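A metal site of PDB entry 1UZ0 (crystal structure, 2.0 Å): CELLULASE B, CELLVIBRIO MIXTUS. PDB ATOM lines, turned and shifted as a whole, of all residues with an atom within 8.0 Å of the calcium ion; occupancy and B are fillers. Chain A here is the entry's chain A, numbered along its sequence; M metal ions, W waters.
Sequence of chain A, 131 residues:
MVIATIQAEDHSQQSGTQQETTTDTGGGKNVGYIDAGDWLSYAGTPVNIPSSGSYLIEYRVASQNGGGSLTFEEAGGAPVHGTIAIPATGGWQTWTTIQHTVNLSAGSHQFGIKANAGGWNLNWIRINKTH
The calcium ion is bound by O of Lys 29 (2.3 Å), OD1 of Asn 123 (2.3 Å), OE1 of Gln 7 (2.3 Å), OE1 of Glu 9 (2.4 Å), water W1 (2.4 Å), O of Asn 123 (2.5 Å) and OE2 of Glu 9 (2.5 Å).
The calcium ion has seven donor atoms within binding distance.
The backbone NH (N) of Ala 8 sits close to the backbone carbonyl oxygen (O) of Asn 123 (3.0 Å).
OD2 of Asp 24 sits at hydrogen-bond distance from ND2 of Asn 123, at 2.7 Å.
The backbone carbonyl oxygen of Arg 60 is in hydrogen-bond range of the backbone NH of Asn 123, 2.8 Å away.
Of the 21 residues printed, 4 come within 4 Å of the calcium ion.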
ATOM      1  N   ILE A   6      12.342   0.706  -5.531  1.00  0.00           N
ATOM      2  CA  ILE A   6      12.854  -0.496  -4.892  1.00  0.00           C
ATOM      3  C   ILE A   6      13.890  -1.113  -5.861  1.00  0.00           C
ATOM      4  O   ILE A   6      13.556  -1.514  -6.971  1.00  0.00           O
ATOM      5  CB  ILE A   6      11.706  -1.519  -4.627  1.00  0.00           C
ATOM      6  CG1 ILE A   6      10.668  -0.966  -3.636  1.00  0.00           C
ATOM      7  CG2 ILE A   6      12.272  -2.791  -4.001  1.00  0.00           C
ATOM      8  CD1 ILE A   6       9.485  -1.819  -3.485  1.00  0.00           C
ATOM      9  N   GLN A   7      15.150  -1.164  -5.423  1.00  0.00           N
ATOM     10  CA  GLN A   7      16.196  -1.886  -6.175  1.00  0.00           C
ATOM     11  C   GLN A   7      15.880  -3.344  -6.138  1.00  0.00           C
ATOM     12  O   GLN A   7      15.553  -3.874  -5.075  1.00  0.00           O
ATOM     13  CB  GLN A   7      17.590  -1.572  -5.603  1.00  0.00           C
ATOM     14  CG  GLN A   7      17.958  -0.122  -5.718  1.00  0.00           C
ATOM     15  CD  GLN A   7      18.198   0.264  -7.161  1.00  0.00           C
ATOM     16  OE1 GLN A   7      18.575  -0.586  -7.960  1.00  0.00           O
ATOM     17  NE2 GLN A   7      17.974   1.526  -7.505  1.00  0.00           N
ATOM     18  N   ALA A   8      15.887  -3.998  -7.319  1.00  0.00           N
ATOM     19  CA  ALA A   8      15.505  -5.400  -7.392  1.00  0.00           C
ATOM     20  C   ALA A   8      16.290  -6.314  -6.420  1.00  0.00           C
ATOM     21  O   ALA A   8      15.764  -7.300  -5.877  1.00  0.00           O
ATOM     22  CB  ALA A   8      15.685  -5.914  -8.830  1.00  0.00           C
ATOM     23  N   GLU A   9      17.569  -5.987  -6.300  1.00  0.00           N
ATOM     24  CA  GLU A   9      18.570  -6.726  -5.487  1.00  0.00           C
ATOM     25  C   GLU A   9      18.378  -6.536  -3.996  1.00  0.00           C
ATOM     26  O   GLU A   9      19.042  -7.197  -3.209  1.00  0.00           O
ATOM     27  CB  GLU A   9      20.014  -6.319  -5.859  1.00  0.00           C
ATOM     28  CG  GLU A   9      20.375  -4.857  -5.633  1.00  0.00           C
ATOM     29  CD  GLU A   9      20.079  -3.921  -6.845  1.00  0.00           C
ATOM     30  OE1 GLU A   9      19.108  -4.113  -7.603  1.00  0.00           O
ATOM     31  OE2 GLU A   9      20.810  -2.922  -7.024  1.00  0.00           O
ATOM     32  N   ASP A  10      17.426  -5.682  -3.576  1.00  0.00           N
ATOM     33  CA  ASP A  10      17.119  -5.543  -2.157  1.00  0.00           C
ATOM     34  C   ASP A  10      16.010  -6.398  -1.639  1.00  0.00           C
ATOM     35  O   ASP A  10      15.372  -6.080  -0.661  1.00  0.00           O
ATOM     36  CB  ASP A  10      16.840  -4.084  -1.819  1.00  0.00           C
ATOM     37  CG  ASP A  10      18.072  -3.222  -1.963  1.00  0.00           C
ATOM     38  OD1 ASP A  10      19.184  -3.775  -1.980  1.00  0.00           O
ATOM     39  OD2 ASP A  10      18.014  -1.983  -2.140  1.00  0.00           O
ATOM     40  N   GLU A  20      23.904  -9.726 -10.297  1.00  0.00           N
ATOM     41  CA  GLU A  20      25.069  -9.433 -11.112  1.00  0.00           C
ATOM     42  C   GLU A  20      25.227  -7.910 -11.207  1.00  0.00           C
ATOM     43  O   GLU A  20      24.305  -7.149 -10.889  1.00  0.00           O
ATOM     44  CB  GLU A  20      24.934 -10.041 -12.521  1.00  0.00           C
ATOM     45  CG  GLU A  20      23.767  -9.509 -13.360  1.00  0.00           C
ATOM     46  CD  GLU A  20      23.454 -10.321 -14.625  1.00  0.00           C
ATOM     47  OE1 GLU A  20      24.239 -11.252 -15.002  1.00  0.00           O
ATOM     48  OE2 GLU A  20      22.403 -10.014 -15.281  1.00  0.00           O
ATOM     49  N   THR A  22      25.252  -4.397 -12.873  1.00  0.00           N
ATOM     50  CA  THR A  22      24.610  -3.818 -14.026  1.00  0.00           C
ATOM     51  C   THR A  22      25.420  -2.657 -14.619  1.00  0.00           C
ATOM     52  O   THR A  22      26.063  -1.911 -13.892  1.00  0.00           O
ATOM     53  CB  THR A  22      23.186  -3.349 -13.708  1.00  0.00           C
ATOM     54  OG1 THR A  22      22.568  -2.912 -14.928  1.00  0.00           O
ATOM     55  CG2 THR A  22      23.171  -2.102 -12.766  1.00  0.00           C
ATOM     56  N   ASP A  24      23.669  -0.471 -16.521  1.00  0.00           N
ATOM     57  CA  ASP A  24      22.633   0.527 -16.650  1.00  0.00           C
ATOM     58  C   ASP A  24      23.105   1.787 -15.998  1.00  0.00           C
ATOM     59  O   ASP A  24      24.015   1.756 -15.188  1.00  0.00           O
ATOM     60  CB  ASP A  24      21.356   0.037 -15.961  1.00  0.00           C
ATOM     61  CG  ASP A  24      20.102   0.794 -16.367  1.00  0.00           C
ATOM     62  OD1 ASP A  24      20.131   1.541 -17.395  1.00  0.00           O
ATOM     63  OD2 ASP A  24      19.000   0.684 -15.724  1.00  0.00           O
ATOM     64  N   THR A  25      22.458   2.885 -16.333  1.00  0.00           N
ATOM     65  CA  THR A  25      22.703   4.177 -15.713  1.00  0.00           C
ATOM     66  C   THR A  25      22.589   4.087 -14.214  1.00  0.00           C
ATOM     67  O   THR A  25      21.585   3.535 -13.729  1.00  0.00           O
ATOM     68  CB  THR A  25      21.673   5.197 -16.220  1.00  0.00           C
ATOM     69  OG1 THR A  25      21.676   5.164 -17.640  1.00  0.00           O
ATOM     70  CG2 THR A  25      22.092   6.594 -15.878  1.00  0.00           C
ATOM     71  N   GLY A  26      23.601   4.601 -13.498  1.00  0.00           N
ATOM     72  CA  GLY A  26      23.617   4.573 -12.053  1.00  0.00           C
ATOM     73  C   GLY A  26      24.343   3.399 -11.450  1.00  0.00           C
ATOM     74  O   GLY A  26      24.684   3.415 -10.275  1.00  0.00           O
ATOM     75  N   GLY A  27      24.610   2.365 -12.253  1.00  0.00           N
ATOM     76  CA  GLY A  27      25.386   1.243 -11.779  1.00  0.00           C
ATOM     77  C   GLY A  27      24.666   0.432 -10.709  1.00  0.00           C
ATOM     78  O   GLY A  27      23.436   0.362 -10.684  1.00  0.00           O
ATOM     79  N   GLY A  28      25.469  -0.233  -9.889  1.00  0.00           N
ATOM     80  CA  GLY A  28      25.000  -1.162  -8.854  1.00  0.00           C
ATOM     81  C   GLY A  28      24.713  -2.511  -9.471  1.00  0.00           C
ATOM     82  O   GLY A  28      25.513  -3.039 -10.253  1.00  0.00           O
ATOM     83  N   LYS A  29      23.593  -3.117  -9.116  1.00  0.00           N
ATOM     84  CA  LYS A  29      23.346  -4.502  -9.535  1.00  0.00           C
ATOM     85  C   LYS A  29      21.959  -4.695 -10.158  1.00  0.00           C
ATOM     86  O   LYS A  29      21.056  -3.858 -10.002  1.00  0.00           O
ATOM     87  CB  LYS A  29      23.464  -5.431  -8.298  1.00  0.00           C
ATOM     88  CG  LYS A  29      24.846  -5.444  -7.594  1.00  0.00           C
ATOM     89  CD  LYS A  29      24.825  -6.421  -6.411  1.00  0.00           C
ATOM     90  CE  LYS A  29      26.141  -6.514  -5.643  1.00  0.00           C
ATOM     91  NZ  LYS A  29      27.268  -6.792  -6.584  1.00  0.00           N
ATOM     92  N   ASN A  30      21.806  -5.803 -10.868  1.00  0.00           N
ATOM     93  CA  ASN A  30      20.489  -6.249 -11.306  1.00  0.00           C
ATOM     94  C   ASN A  30      20.266  -7.669 -10.864  1.00  0.00           C
ATOM     95  O   ASN A  30      21.214  -8.356 -10.481  1.00  0.00           O
ATOM     96  CB  ASN A  30      20.274  -6.021 -12.817  1.00  0.00           C
ATOM     97  CG  ASN A  30      21.110  -6.919 -13.687  1.00  0.00           C
ATOM     98  OD1 ASN A  30      20.741  -8.105 -13.983  1.00  0.00           O
ATOM     99  ND2 ASN A  30      22.271  -6.409 -14.078  1.00  0.00           N
ATOM    100  N   VAL A  31      19.010  -8.072 -10.823  1.00  0.00           N
ATOM    101  CA  VAL A  31      18.637  -9.443 -10.703  1.00  0.00           C
ATOM    102  C   VAL A  31      18.563 -10.056 -12.103  1.00  0.00           C
ATOM    103  O   VAL A  31      17.946  -9.486 -13.046  1.00  0.00           O
ATOM    104  CB  VAL A  31      17.298  -9.605  -9.978  1.00  0.00           C
ATOM    105  CG1 VAL A  31      16.876 -11.081  -9.955  1.00  0.00           C
ATOM    106  CG2 VAL A  31      17.329  -9.114  -8.554  1.00  0.00           C
ATOM    107  N   ARG A  60      12.441  -1.516 -14.584  1.00  0.00           N
ATOM    108  CA  ARG A  60      13.631  -1.281 -15.359  1.00  0.00           C
ATOM    109  C   ARG A  60      14.151  -2.650 -15.716  1.00  0.00           C
ATOM    110  O   ARG A  60      14.621  -3.441 -14.839  1.00  0.00           O
ATOM    111  CB  ARG A  60      14.612  -0.418 -14.560  1.00  0.00           C
ATOM    112  CG  ARG A  60      15.820   0.077 -15.351  1.00  0.00           C
ATOM    113  CD  ARG A  60      15.492   1.065 -16.390  1.00  0.00           C
ATOM    114  NE  ARG A  60      16.696   1.587 -17.032  1.00  0.00           N
ATOM    115  CZ  ARG A  60      16.656   2.401 -18.092  1.00  0.00           C
ATOM    116  NH1 ARG A  60      15.487   2.714 -18.629  1.00  0.00           N
ATOM    117  NH2 ARG A  60      17.807   2.816 -18.655  1.00  0.00           N
ATOM    118  N   TRP A  95      18.741  -1.642 -21.455  1.00  0.00           N
ATOM    119  CA  TRP A  95      17.661  -1.355 -20.494  1.00  0.00           C
ATOM    120  C   TRP A  95      16.600  -0.421 -21.040  1.00  0.00           C
ATOM    121  O   TRP A  95      16.879   0.484 -21.844  1.00  0.00           O
ATOM    122  CB  TRP A  95      18.241  -0.785 -19.217  1.00  0.00           C
ATOM    123  CG  TRP A  95      19.185  -1.750 -18.601  1.00  0.00           C
ATOM    124  CD1 TRP A  95      20.529  -1.848 -18.800  1.00  0.00           C
ATOM    125  CD2 TRP A  95      18.846  -2.805 -17.689  1.00  0.00           C
ATOM    126  NE1 TRP A  95      21.050  -2.887 -18.063  1.00  0.00           N
ATOM    127  CE2 TRP A  95      20.029  -3.498 -17.373  1.00  0.00           C
ATOM    128  CE3 TRP A  95      17.660  -3.218 -17.095  1.00  0.00           C
ATOM    129  CZ2 TRP A  95      20.054  -4.608 -16.509  1.00  0.00           C
ATOM    130  CZ3 TRP A  95      17.699  -4.311 -16.202  1.00  0.00           C
ATOM    131  CH2 TRP A  95      18.890  -4.991 -15.957  1.00  0.00           C
ATOM    132  N   LEU A 122      16.015  -7.562 -14.105  1.00  0.00           N
ATOM    133  CA  LEU A 122      15.307  -6.462 -13.377  1.00  0.00           C
ATOM    134  C   LEU A 122      16.283  -5.622 -12.585  1.00  0.00           C
ATOM    135  O   LEU A 122      17.024  -6.168 -11.761  1.00  0.00           O
ATOM    136  CB  LEU A 122      14.271  -7.073 -12.425  1.00  0.00           C
ATOM    137  CG  LEU A 122      13.300  -6.076 -11.746  1.00  0.00           C
ATOM    138  CD1 LEU A 122      12.444  -5.299 -12.775  1.00  0.00           C
ATOM    139  CD2 LEU A 122      12.412  -6.862 -10.756  1.00  0.00           C
ATOM    140  N   ASN A 123      16.362  -4.321 -12.873  1.00  0.00           N
ATOM    141  CA  ASN A 123      17.249  -3.433 -12.159  1.00  0.00           C
ATOM    142  C   ASN A 123      16.587  -2.849 -10.888  1.00  0.00           C
ATOM    143  O   ASN A 123      17.164  -2.852  -9.767  1.00  0.00           O
ATOM    144  CB  ASN A 123      17.798  -2.387 -13.099  1.00  0.00           C
ATOM    145  CG  ASN A 123      18.875  -1.471 -12.473  1.00  0.00           C
ATOM    146  OD1 ASN A 123      19.364  -1.706 -11.389  1.00  0.00           O
ATOM    147  ND2 ASN A 123      19.252  -0.404 -13.224  1.00  0.00           N
ATOM    148  N   TRP A 124      15.395  -2.318 -11.082  1.00  0.00           N
ATOM    149  CA  TRP A 124      14.628  -1.688  -9.998  1.00  0.00           C
ATOM    150  C   TRP A 124      13.157  -1.614 -10.422  1.00  0.00           C
ATOM    151  O   TRP A 124      12.849  -1.897 -11.573  1.00  0.00           O
ATOM    152  CB  TRP A 124      15.184  -0.288  -9.615  1.00  0.00           C
ATOM    153  CG  TRP A 124      15.523   0.664 -10.776  1.00  0.00           C
ATOM    154  CD1 TRP A 124      16.770   0.971 -11.237  1.00  0.00           C
ATOM    155  CD2 TRP A 124      14.612   1.449 -11.563  1.00  0.00           C
ATOM    156  NE1 TRP A 124      16.673   1.905 -12.250  1.00  0.00           N
ATOM    157  CE2 TRP A 124      15.366   2.193 -12.492  1.00  0.00           C
ATOM    158  CE3 TRP A 124      13.217   1.587 -11.571  1.00  0.00           C
ATOM    159  CZ2 TRP A 124      14.768   3.037 -13.479  1.00  0.00           C
ATOM    160  CZ3 TRP A 124      12.622   2.455 -12.523  1.00  0.00           C
ATOM    161  CH2 TRP A 124      13.399   3.181 -13.455  1.00  0.00           C
ATOM    162  N   ILE A 125      12.299  -1.255  -9.453  1.00  0.00           N
ATOM    163  CA  ILE A 125      10.853  -1.059  -9.612  1.00  0.00           C
ATOM    164  C   ILE A 125      10.528   0.281  -9.000  1.00  0.00           C
ATOM    165  O   ILE A 125      11.098   0.652  -8.006  1.00  0.00           O
ATOM    166  CB  ILE A 125      10.132  -2.169  -8.837  1.00  0.00           C
ATOM    167  CG1 ILE A 125      10.556  -3.533  -9.393  1.00  0.00           C
ATOM    168  CG2 ILE A 125       8.660  -2.068  -8.905  1.00  0.00           C
ATOM    169  CD1 ILE A 125      10.924  -4.437  -8.221  1.00  0.00           C
HETATM  170 CA    CA M   1      19.570  -2.324  -9.159  1.00  0.00          CA
HETATM  171  O   HOH W   1      21.466  -0.821  -8.980  1.00  0.00           O
